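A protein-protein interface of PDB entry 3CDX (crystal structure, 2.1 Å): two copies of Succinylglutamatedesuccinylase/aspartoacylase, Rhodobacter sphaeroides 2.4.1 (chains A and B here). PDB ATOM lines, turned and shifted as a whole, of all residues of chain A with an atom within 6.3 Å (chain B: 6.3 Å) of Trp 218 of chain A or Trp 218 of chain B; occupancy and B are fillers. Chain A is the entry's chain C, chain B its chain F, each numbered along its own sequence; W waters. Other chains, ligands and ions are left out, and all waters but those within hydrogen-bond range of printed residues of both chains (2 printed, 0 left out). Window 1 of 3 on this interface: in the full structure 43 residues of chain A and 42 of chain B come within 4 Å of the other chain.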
ATOM      1  N   ALA A 151     -30.894  25.328   4.353  1.00  0.00           N
ATOM      2  CA  ALA A 151     -32.174  24.684   4.577  1.00  0.00           C
ATOM      3  C   ALA A 151     -32.420  24.270   6.048  1.00  0.00           C
ATOM      4  O   ALA A 151     -33.467  23.692   6.335  1.00  0.00           O
ATOM      5  CB  ALA A 151     -32.329  23.469   3.628  1.00  0.00           C
ATOM      6  N   GLY A 152     -31.475  24.563   6.967  1.00  0.00           N
ATOM      7  CA  GLY A 152     -31.612  24.222   8.385  1.00  0.00           C
ATOM      8  C   GLY A 152     -31.986  22.774   8.651  1.00  0.00           C
ATOM      9  O   GLY A 152     -31.324  21.874   8.158  1.00  0.00           O
ATOM     10  N   HIS A 153     -33.055  22.552   9.423  1.00  0.00           N
ATOM     11  CA  HIS A 153     -33.568  21.182   9.665  1.00  0.00           C
ATOM     12  C   HIS A 153     -34.508  20.635   8.595  1.00  0.00           C
ATOM     13  O   HIS A 153     -34.825  19.460   8.607  1.00  0.00           O
ATOM     14  CB  HIS A 153     -34.211  21.039  11.064  1.00  0.00           C
ATOM     15  CG  HIS A 153     -33.225  21.153  12.185  1.00  0.00           C
ATOM     16  ND1 HIS A 153     -32.726  22.365  12.620  1.00  0.00           N
ATOM     17  CD2 HIS A 153     -32.605  20.206  12.932  1.00  0.00           C
ATOM     18  CE1 HIS A 153     -31.872  22.160  13.606  1.00  0.00           C
ATOM     19  NE2 HIS A 153     -31.780  20.860  13.816  1.00  0.00           N
ATOM     20  N   SER A 154     -34.936  21.472   7.661  1.00  0.00           N
ATOM     21  CA  SER A 154     -35.965  21.091   6.660  1.00  0.00           C
ATOM     22  C   SER A 154     -35.464  20.212   5.485  1.00  0.00           C
ATOM     23  O   SER A 154     -36.156  19.279   5.044  1.00  0.00           O
ATOM     24  CB  SER A 154     -36.658  22.361   6.125  1.00  0.00           C
ATOM     25  OG  SER A 154     -37.329  23.066   7.172  1.00  0.00           O
ATOM     26  N   TYR A 155     -34.270  20.517   4.974  1.00  0.00           N
ATOM     27  CA  TYR A 155     -33.704  19.845   3.785  1.00  0.00           C
ATOM     28  C   TYR A 155     -32.210  19.863   3.877  1.00  0.00           C
ATOM     29  O   TYR A 155     -31.668  20.503   4.764  1.00  0.00           O
ATOM     30  CB  TYR A 155     -34.089  20.595   2.498  1.00  0.00           C
ATOM     31  CG  TYR A 155     -35.575  20.689   2.357  1.00  0.00           C
ATOM     32  CD1 TYR A 155     -36.286  19.575   1.972  1.00  0.00           C
ATOM     33  CD2 TYR A 155     -36.274  21.873   2.650  1.00  0.00           C
ATOM     34  CE1 TYR A 155     -37.625  19.597   1.864  1.00  0.00           C
ATOM     35  CE2 TYR A 155     -37.675  21.908   2.531  1.00  0.00           C
ATOM     36  CZ  TYR A 155     -38.325  20.740   2.136  1.00  0.00           C
ATOM     37  OH  TYR A 155     -39.682  20.639   1.988  1.00  0.00           O
ATOM     38  N   ASP A 156     -31.537  19.163   2.968  1.00  0.00           N
ATOM     39  CA  ASP A 156     -30.214  19.594   2.596  1.00  0.00           C
ATOM     40  C   ASP A 156     -30.327  20.463   1.328  1.00  0.00           C
ATOM     41  O   ASP A 156     -31.271  20.325   0.551  1.00  0.00           O
ATOM     42  CB  ASP A 156     -29.270  18.428   2.335  1.00  0.00           C
ATOM     43  CG  ASP A 156     -27.804  18.825   2.476  1.00  0.00           C
ATOM     44  OD1 ASP A 156     -27.494  19.918   3.009  1.00  0.00           O
ATOM     45  OD2 ASP A 156     -26.946  18.033   2.061  1.00  0.00           O
ATOM     46  N   SER A 157     -29.344  21.345   1.115  1.00  0.00           N
ATOM     47  CA  SER A 157     -29.301  22.130  -0.123  1.00  0.00           C
ATOM     48  C   SER A 157     -27.906  22.019  -0.750  1.00  0.00           C
ATOM     49  O   SER A 157     -26.895  21.924  -0.044  1.00  0.00           O
ATOM     50  CB  SER A 157     -29.723  23.585   0.133  1.00  0.00           C
ATOM     51  OG  SER A 157     -28.858  24.239   1.047  1.00  0.00           O
ATOM     52  N   GLY A 216     -26.397  24.505   2.705  1.00  0.00           N
ATOM     53  CA  GLY A 216     -26.469  23.226   3.425  1.00  0.00           C
ATOM     54  C   GLY A 216     -27.830  22.955   4.069  1.00  0.00           C
ATOM     55  O   GLY A 216     -28.878  23.219   3.474  1.00  0.00           O
ATOM     56  N   GLY A 217     -27.813  22.409   5.279  1.00  0.00           N
ATOM     57  CA  GLY A 217     -29.025  21.943   5.958  1.00  0.00           C
ATOM     58  C   GLY A 217     -28.693  20.638   6.660  1.00  0.00           C
ATOM     59  O   GLY A 217     -27.549  20.450   7.118  1.00  0.00           O
ATOM     60  N   TRP A 218     -29.677  19.732   6.718  1.00  0.00           N
ATOM     61  CA  TRP A 218     -29.589  18.466   7.456  1.00  0.00           C
ATOM     62  C   TRP A 218     -29.247  18.684   8.944  1.00  0.00           C
ATOM     63  O   TRP A 218     -28.603  17.820   9.551  1.00  0.00           O
ATOM     64  CB  TRP A 218     -28.555  17.512   6.789  1.00  0.00           C
ATOM     65  CG  TRP A 218     -29.121  16.641   5.705  1.00  0.00           C
ATOM     66  CD1 TRP A 218     -30.449  16.554   5.331  1.00  0.00           C
ATOM     67  CD2 TRP A 218     -28.413  15.707   4.879  1.00  0.00           C
ATOM     68  NE1 TRP A 218     -30.600  15.633   4.341  1.00  0.00           N
ATOM     69  CE2 TRP A 218     -29.366  15.097   4.032  1.00  0.00           C
ATOM     70  CE3 TRP A 218     -27.076  15.316   4.781  1.00  0.00           C
ATOM     71  CZ2 TRP A 218     -29.019  14.106   3.098  1.00  0.00           C
ATOM     72  CZ3 TRP A 218     -26.725  14.347   3.824  1.00  0.00           C
ATOM     73  CH2 TRP A 218     -27.688  13.752   3.002  1.00  0.00           C
ATOM     74  N   GLY A 219     -29.588  19.858   9.495  1.00  0.00           N
ATOM     75  CA  GLY A 219     -29.337  20.146  10.912  1.00  0.00           C
ATOM     76  C   GLY A 219     -27.839  20.202  11.258  1.00  0.00           C
ATOM     77  O   GLY A 219     -27.466  20.310  12.447  1.00  0.00           O
ATOM     78  N   ARG A 220     -26.990  20.157  10.231  1.00  0.00           N
ATOM     79  CA  ARG A 220     -25.512  20.071  10.445  1.00  0.00           C
ATOM     80  C   ARG A 220     -24.747  21.215   9.803  1.00  0.00           C
ATOM     81  O   ARG A 220     -25.338  22.023   9.075  1.00  0.00           O
ATOM     82  CB  ARG A 220     -24.964  18.695   9.991  1.00  0.00           C
ATOM     83  CG  ARG A 220     -25.183  18.277   8.494  1.00  0.00           C
ATOM     84  CD  ARG A 220     -24.167  18.913   7.523  1.00  0.00           C
ATOM     85  NE  ARG A 220     -24.153  18.280   6.175  1.00  0.00           N
ATOM     86  CZ  ARG A 220     -24.927  18.635   5.135  1.00  0.00           C
ATOM     87  NH1 ARG A 220     -25.829  19.631   5.242  1.00  0.00           N
ATOM     88  NH2 ARG A 220     -24.809  17.991   3.967  1.00  0.00           N
ATOM     89  N   VAL A 221     -23.439  21.298  10.083  1.00  0.00           N
ATOM     90  CA  VAL A 221     -22.551  22.241   9.380  1.00  0.00           C
ATOM     91  C   VAL A 221     -21.864  21.577   8.179  1.00  0.00           C
ATOM     92  O   VAL A 221     -21.250  20.531   8.321  1.00  0.00           O
ATOM     93  CB  VAL A 221     -21.463  22.804  10.312  1.00  0.00           C
ATOM     94  CG1 VAL A 221     -20.529  23.690   9.551  1.00  0.00           C
ATOM     95  CG2 VAL A 221     -22.091  23.599  11.458  1.00  0.00           C
ATOM     96  N   TYR A 283     -29.362  12.478  -3.742  1.00  0.00           N
ATOM     97  CA  TYR A 283     -29.056  13.606  -2.879  1.00  0.00           C
ATOM     98  C   TYR A 283     -29.002  14.906  -3.685  1.00  0.00           C
ATOM     99  O   TYR A 283     -28.951  14.886  -4.909  1.00  0.00           O
ATOM    100  CB  TYR A 283     -27.698  13.407  -2.234  1.00  0.00           C
ATOM    101  CG  TYR A 283     -27.608  12.279  -1.239  1.00  0.00           C
ATOM    102  CD1 TYR A 283     -28.625  12.057  -0.283  1.00  0.00           C
ATOM    103  CD2 TYR A 283     -26.499  11.418  -1.242  1.00  0.00           C
ATOM    104  CE1 TYR A 283     -28.542  11.004   0.652  1.00  0.00           C
ATOM    105  CE2 TYR A 283     -26.405  10.353  -0.305  1.00  0.00           C
ATOM    106  CZ  TYR A 283     -27.412  10.160   0.629  1.00  0.00           C
ATOM    107  OH  TYR A 283     -27.288   9.131   1.551  1.00  0.00           O
ATOM    108  N   GLY A 321     -32.968  18.532  -1.206  1.00  0.00           N
ATOM    109  CA  GLY A 321     -33.283  17.108  -1.041  1.00  0.00           C
ATOM    110  C   GLY A 321     -33.912  16.919   0.331  1.00  0.00           C
ATOM    111  O   GLY A 321     -33.673  17.729   1.242  1.00  0.00           O
ATOM    112  N   ALA A 322     -34.697  15.843   0.459  1.00  0.00           N
ATOM    113  CA  ALA A 322     -35.239  15.347   1.711  1.00  0.00           C
ATOM    114  C   ALA A 322     -34.371  15.608   2.963  1.00  0.00           C
ATOM    115  O   ALA A 322     -33.158  15.289   2.973  1.00  0.00           O
ATOM    116  CB  ALA A 322     -35.519  13.833   1.578  1.00  0.00           C
ATOM    117  N   GLY A 323     -34.999  16.161   4.001  1.00  0.00           N
ATOM    118  CA  GLY A 323     -34.340  16.415   5.295  1.00  0.00           C
ATOM    119  C   GLY A 323     -34.640  15.282   6.271  1.00  0.00           C
ATOM    120  O   GLY A 323     -33.969  14.248   6.235  1.00  0.00           O
ATOM    121  N   PRO A 324     -35.673  15.458   7.119  1.00  0.00           N
ATOM    122  CA  PRO A 324     -36.128  14.440   8.063  1.00  0.00           C
ATOM    123  C   PRO A 324     -36.501  13.125   7.385  1.00  0.00           C
ATOM    124  O   PRO A 324     -37.142  13.134   6.322  1.00  0.00           O
ATOM    125  CB  PRO A 324     -37.392  15.052   8.706  1.00  0.00           C
ATOM    126  CG  PRO A 324     -37.606  16.375   8.072  1.00  0.00           C
ATOM    127  CD  PRO A 324     -36.469  16.698   7.164  1.00  0.00           C
ATOM    128  N   ALA B 151     -27.002   6.992  14.254  1.00  0.00           N
ATOM    129  CA  ALA B 151     -26.792   8.085  15.210  1.00  0.00           C
ATOM    130  C   ALA B 151     -27.980   9.052  15.305  1.00  0.00           C
ATOM    131  O   ALA B 151     -27.905  10.055  16.028  1.00  0.00           O
ATOM    132  CB  ALA B 151     -25.532   8.819  14.861  1.00  0.00           C
ATOM    133  N   GLY B 152     -29.051   8.761  14.554  1.00  0.00           N
ATOM    134  CA  GLY B 152     -30.292   9.539  14.570  1.00  0.00           C
ATOM    135  C   GLY B 152     -30.010  11.029  14.381  1.00  0.00           C
ATOM    136  O   GLY B 152     -29.332  11.447  13.405  1.00  0.00           O
ATOM    137  N   HIS B 153     -30.470  11.813  15.349  1.00  0.00           N
ATOM    138  CA  HIS B 153     -30.226  13.261  15.349  1.00  0.00           C
ATOM    139  C   HIS B 153     -28.915  13.697  15.970  1.00  0.00           C
ATOM    140  O   HIS B 153     -28.564  14.855  15.867  1.00  0.00           O
ATOM    141  CB  HIS B 153     -31.397  14.018  15.999  1.00  0.00           C
ATOM    142  CG  HIS B 153     -32.620  14.067  15.146  1.00  0.00           C
ATOM    143  ND1 HIS B 153     -33.593  13.091  15.182  1.00  0.00           N
ATOM    144  CD2 HIS B 153     -33.034  14.980  14.230  1.00  0.00           C
ATOM    145  CE1 HIS B 153     -34.555  13.405  14.327  1.00  0.00           C
ATOM    146  NE2 HIS B 153     -34.239  14.546  13.741  1.00  0.00           N
ATOM    147  N   SER B 154     -28.162  12.778  16.580  1.00  0.00           N
ATOM    148  CA  SER B 154     -27.009  13.182  17.429  1.00  0.00           C
ATOM    149  C   SER B 154     -25.692  13.391  16.662  1.00  0.00           C
ATOM    150  O   SER B 154     -24.891  14.289  17.001  1.00  0.00           O
ATOM    151  CB  SER B 154     -26.818  12.182  18.567  1.00  0.00           C
ATOM    152  OG  SER B 154     -27.953  12.170  19.474  1.00  0.00           O
ATOM    153  N   TYR B 155     -25.469  12.554  15.643  1.00  0.00           N
ATOM    154  CA  TYR B 155     -24.210  12.489  14.895  1.00  0.00           C
ATOM    155  C   TYR B 155     -24.540  12.029  13.499  1.00  0.00           C
ATOM    156  O   TYR B 155     -25.697  11.706  13.217  1.00  0.00           O
ATOM    157  CB  TYR B 155     -23.280  11.435  15.517  1.00  0.00           C
ATOM    158  CG  TYR B 155     -22.937  11.787  16.945  1.00  0.00           C
ATOM    159  CD1 TYR B 155     -22.203  12.924  17.202  1.00  0.00           C
ATOM    160  CD2 TYR B 155     -23.384  11.015  18.024  1.00  0.00           C
ATOM    161  CE1 TYR B 155     -21.900  13.302  18.461  1.00  0.00           C
ATOM    162  CE2 TYR B 155     -23.062  11.381  19.350  1.00  0.00           C
ATOM    163  CZ  TYR B 155     -22.319  12.539  19.535  1.00  0.00           C
ATOM    164  OH  TYR B 155     -21.952  13.025  20.757  1.00  0.00           O
ATOM    165  N   ASP B 156     -23.538  11.985  12.633  1.00  0.00           N
ATOM    166  CA  ASP B 156     -23.584  11.073  11.514  1.00  0.00           C
ATOM    167  C   ASP B 156     -22.665   9.920  11.880  1.00  0.00           C
ATOM    168  O   ASP B 156     -21.784  10.090  12.725  1.00  0.00           O
ATOM    169  CB  ASP B 156     -23.093  11.702  10.198  1.00  0.00           C
ATOM    170  CG  ASP B 156     -23.652  10.968   8.982  1.00  0.00           C
ATOM    171  OD1 ASP B 156     -24.603  10.178   9.176  1.00  0.00           O
ATOM    172  OD2 ASP B 156     -23.137  11.121   7.856  1.00  0.00           O
ATOM    173  N   SER B 157     -22.872   8.760  11.250  1.00  0.00           N
ATOM    174  CA  SER B 157     -22.004   7.600  11.432  1.00  0.00           C
ATOM    175  C   SER B 157     -21.652   6.976  10.077  1.00  0.00           C
ATOM    176  O   SER B 157     -22.457   6.990   9.130  1.00  0.00           O
ATOM    177  CB  SER B 157     -22.619   6.540  12.361  1.00  0.00           C
ATOM    178  OG  SER B 157     -23.840   6.004  11.846  1.00  0.00           O
ATOM    179  N   GLY B 216     -25.929   5.579   9.786  1.00  0.00           N
ATOM    180  CA  GLY B 216     -26.139   6.980   9.429  1.00  0.00           C
ATOM    181  C   GLY B 216     -26.459   7.930  10.594  1.00  0.00           C
ATOM    182  O   GLY B 216     -25.843   7.881  11.670  1.00  0.00           O
ATOM    183  N   GLY B 217     -27.460   8.774  10.376  1.00  0.00           N
ATOM    184  CA  GLY B 217     -27.780   9.841  11.297  1.00  0.00           C
ATOM    185  C   GLY B 217     -28.029  11.129  10.535  1.00  0.00           C
ATOM    186  O   GLY B 217     -28.579  11.111   9.420  1.00  0.00           O
ATOM    187  N   TRP B 218     -27.625  12.236  11.143  1.00  0.00           N
ATOM    188  CA  TRP B 218     -27.868  13.588  10.618  1.00  0.00           C
ATOM    189  C   TRP B 218     -29.354  13.868  10.422  1.00  0.00           C
ATOM    190  O   TRP B 218     -29.724  14.725   9.606  1.00  0.00           O
ATOM    191  CB  TRP B 218     -27.078  13.831   9.321  1.00  0.00           C
ATOM    192  CG  TRP B 218     -25.675  14.427   9.505  1.00  0.00           C
ATOM    193  CD1 TRP B 218     -25.090  14.885  10.686  1.00  0.00           C
ATOM    194  CD2 TRP B 218     -24.742  14.727   8.460  1.00  0.00           C
ATOM    195  NE1 TRP B 218     -23.831  15.423  10.419  1.00  0.00           N
ATOM    196  CE2 TRP B 218     -23.588  15.319   9.071  1.00  0.00           C
ATOM    197  CE3 TRP B 218     -24.756  14.534   7.070  1.00  0.00           C
ATOM    198  CZ2 TRP B 218     -22.463  15.731   8.319  1.00  0.00           C
ATOM    199  CZ3 TRP B 218     -23.661  14.936   6.324  1.00  0.00           C
ATOM    200  CH2 TRP B 218     -22.513  15.535   6.951  1.00  0.00           C
ATOM    201  N   GLY B 219     -30.201  13.146  11.173  1.00  0.00           N
ATOM    202  CA  GLY B 219     -31.671  13.309  11.132  1.00  0.00           C
ATOM    203  C   GLY B 219     -32.284  12.893   9.799  1.00  0.00           C
ATOM    204  O   GLY B 219     -33.477  13.139   9.554  1.00  0.00           O
ATOM    205  N   ARG B 220     -31.479  12.264   8.938  1.00  0.00           N
ATOM    206  CA  ARG B 220     -31.872  11.969   7.559  1.00  0.00           C
ATOM    207  C   ARG B 220     -31.785  10.486   7.242  1.00  0.00           C
ATOM    208  O   ARG B 220     -31.332   9.696   8.072  1.00  0.00           O
ATOM    209  CB  ARG B 220     -31.057  12.778   6.534  1.00  0.00           C
ATOM    210  CG  ARG B 220     -29.492  12.567   6.509  1.00  0.00           C
ATOM    211  CD  ARG B 220     -28.948  11.297   5.809  1.00  0.00           C
ATOM    212  NE  ARG B 220     -27.522  11.452   5.489  1.00  0.00           N
ATOM    213  CZ  ARG B 220     -26.495  11.072   6.273  1.00  0.00           C
ATOM    214  NH1 ARG B 220     -26.714  10.470   7.430  1.00  0.00           N
ATOM    215  NH2 ARG B 220     -25.228  11.320   5.909  1.00  0.00           N
ATOM    216  N   VAL B 221     -32.237  10.122   6.031  1.00  0.00           N
ATOM    217  CA  VAL B 221     -32.050   8.765   5.517  1.00  0.00           C
ATOM    218  C   VAL B 221     -30.789   8.676   4.614  1.00  0.00           C
ATOM    219  O   VAL B 221     -30.680   9.401   3.626  1.00  0.00           O
ATOM    220  CB  VAL B 221     -33.297   8.202   4.786  1.00  0.00           C
ATOM    221  CG1 VAL B 221     -32.953   6.792   4.200  1.00  0.00           C
ATOM    222  CG2 VAL B 221     -34.496   8.106   5.739  1.00  0.00           C
ATOM    223  N   TYR B 283     -15.380  14.706   8.098  1.00  0.00           N
ATOM    224  CA  TYR B 283     -16.601  13.952   8.202  1.00  0.00           C
ATOM    225  C   TYR B 283     -16.246  12.508   8.554  1.00  0.00           C
ATOM    226  O   TYR B 283     -15.080  12.112   8.448  1.00  0.00           O
ATOM    227  CB  TYR B 283     -17.316  13.963   6.864  1.00  0.00           C
ATOM    228  CG  TYR B 283     -17.941  15.273   6.407  1.00  0.00           C
ATOM    229  CD1 TYR B 283     -18.712  16.077   7.273  1.00  0.00           C
ATOM    230  CD2 TYR B 283     -17.848  15.655   5.070  1.00  0.00           C
ATOM    231  CE1 TYR B 283     -19.319  17.247   6.813  1.00  0.00           C
ATOM    232  CE2 TYR B 283     -18.465  16.833   4.598  1.00  0.00           C
ATOM    233  CZ  TYR B 283     -19.202  17.608   5.460  1.00  0.00           C
ATOM    234  OH  TYR B 283     -19.794  18.758   4.954  1.00  0.00           O
ATOM    235  N   GLY B 321     -19.407  11.507  13.653  1.00  0.00           N
ATOM    236  CA  GLY B 321     -19.060  12.875  13.303  1.00  0.00           C
ATOM    237  C   GLY B 321     -20.124  13.796  13.834  1.00  0.00           C
ATOM    238  O   GLY B 321     -21.247  13.351  14.083  1.00  0.00           O
ATOM    239  N   ALA B 322     -19.791  15.068  14.014  1.00  0.00           N
ATOM    240  CA  ALA B 322     -20.705  16.034  14.673  1.00  0.00           C
ATOM    241  C   ALA B 322     -22.048  16.059  13.964  1.00  0.00           C
ATOM    242  O   ALA B 322     -22.109  15.893  12.752  1.00  0.00           O
ATOM    243  CB  ALA B 322     -20.083  17.418  14.695  1.00  0.00           C
ATOM    244  N   GLY B 323     -23.123  16.254  14.723  1.00  0.00           N
ATOM    245  CA  GLY B 323     -24.490  16.263  14.191  1.00  0.00           C
ATOM    246  C   GLY B 323     -24.998  17.680  14.192  1.00  0.00           C
ATOM    247  O   GLY B 323     -24.697  18.449  13.275  1.00  0.00           O
ATOM    248  N   PRO B 324     -25.693  18.081  15.268  1.00  0.00           N
ATOM    249  CA  PRO B 324     -26.210  19.439  15.311  1.00  0.00           C
ATOM    250  C   PRO B 324     -25.087  20.473  15.175  1.00  0.00           C
ATOM    251  O   PRO B 324     -23.971  20.230  15.647  1.00  0.00           O
ATOM    252  CB  PRO B 324     -26.850  19.534  16.708  1.00  0.00           C
ATOM    253  CG  PRO B 324     -26.222  18.422  17.499  1.00  0.00           C
ATOM    254  CD  PRO B 324     -25.977  17.322  16.496  1.00  0.00           C
HETATM  255  O   HOH W   1     -22.310  19.448  12.250  1.00  0.00           O
HETATM  256  O   HOH W   2     -33.820  12.085   4.443  1.00  0.00           O
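The backbone carbonyl oxygen (O) of Gly 152 of chain A sits at hydrogen-bond distance from the backbone NH (N) of Gly 219 of chain A, at 3.0 Å. The backbone NH of Trp 218 of chain A is in hydrogen-bond range of the backbone carbonyl oxygen of Tyr 155 of chain A (2.9 Å). The backbone carbonyl oxygen (O) of Gly 217 of chain A lies within hydrogen-bond range of the guanidinium group (NH1) of Arg 220 of chain A, 2.7 Å away. O of Gly 152 of chain B is in hydrogen-bond range of N of Trp 218 of chain B. The backbone carbonyl oxygen (O) of Gly 152 of chain B lies within hydrogen-bond range of the backbone NH (N) of Gly 219 of chain B (2.9 Å). The backbone carbonyl oxygen (O) of Ser 154 of chain B sits close to the backbone NH (N) of Gly 323 of chain B (3.5 Å).
The backbone carbonyl oxygen of Trp 218 of chain A lies close to the backbone carbonyl oxygen of Trp 218 of chain B, 3.3 Å away. The backbone carbonyl oxygen of Gly 219 of chain A lies close to the backbone carbonyl oxygen of Gly 323 of chain B.
Of the printed residues of chain A, Trp 218 of chain B touches Trp 218 (3.3 Å) and Arg 220 (3.3 Å). Of the printed residues of chain B, Gly 323 of chain A touches Gly 219 (3.5 Å) and Arg 220 (3.3 Å). Printed residues of chain B within 4 Å of Tyr 283 of chain A: Val 221 (3.99 Å). Of the printed residues of chain A, Gly 323 of chain B touches Gly 219 (3.4 Å) and Arg 220 (3.3 Å). The nearest residue of chain A that does not touch Trp 218 of chain B is Val 221 of chain A (5.0 Å).
Trp 218 of chain A touches its own counterpart, Trp 218 of chain B. Gly 219 of chain A touches Gly 323 of chain B, and with the chains exchanged Gly 323 of chain A touches Gly 219 of chain B. Gly 219 of chain A touches Pro 324 of chain B, and with the chains exchanged Pro 324 of chain A touches Gly 219 of chain B. Tyr 283 of chain A touches Val 221 of chain B, but with the chains exchanged Val 221 of chain A does not touch Tyr 283 of chain B (4.1 Å). Positions printed for both chains: 151, 152, 153, 154, 155, 156, 157, 216, 217, 218, 219, 220, 221, 283, 321, 322, 323 and 324. Of the 10 pairs that touch across the chains among the printed residues, 9 have their exchanged pair printed and touching as well.
Trp 218 of chain A touches Arg 220 of chain B (CH2 to NE, 3.4 Å). Pro 324 of chain B touches Gly 219 of chain A (CA to O, 3.2 Å). Trp 218 of chain B touches Arg 220 of chain A (CH2 to NE, 3.3 Å). Gly 323 of chain B touches Arg 220 of chain A (O to CB, 3.3 Å). Val 221 of chain B touches Tyr 283 of chain A. Gly 323 of chain A touches Gly 219 of chain B (O to O, 3.5 Å). O of Gly 323 of chain A touches CB of Arg 220 of chain B (3.3 Å). CA of Pro 324 of chain A touches O of Gly 219 of chain B, 3.3 Å away.
Along chain B the printed residues that touch a printed residue of chain A span positions 218 to 324. Printed residues of chain A that touch a printed residue of chain B: Trp 218, Gly 219, Arg 220, Tyr 283, Gly 323 and Pro 324. Hydrophobic or aromatic side chains of chain A that line the printed part of chain B: Trp 218 and Tyr 283.
Water W1 bridges O of Gly 323 of chain B (2.8 Å) and N of Val 221 of chain A (3.1 Å). Water W2 lies within hydrogen-bond range of O of Gly 323 of chain A and N of Val 221 of chain B.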
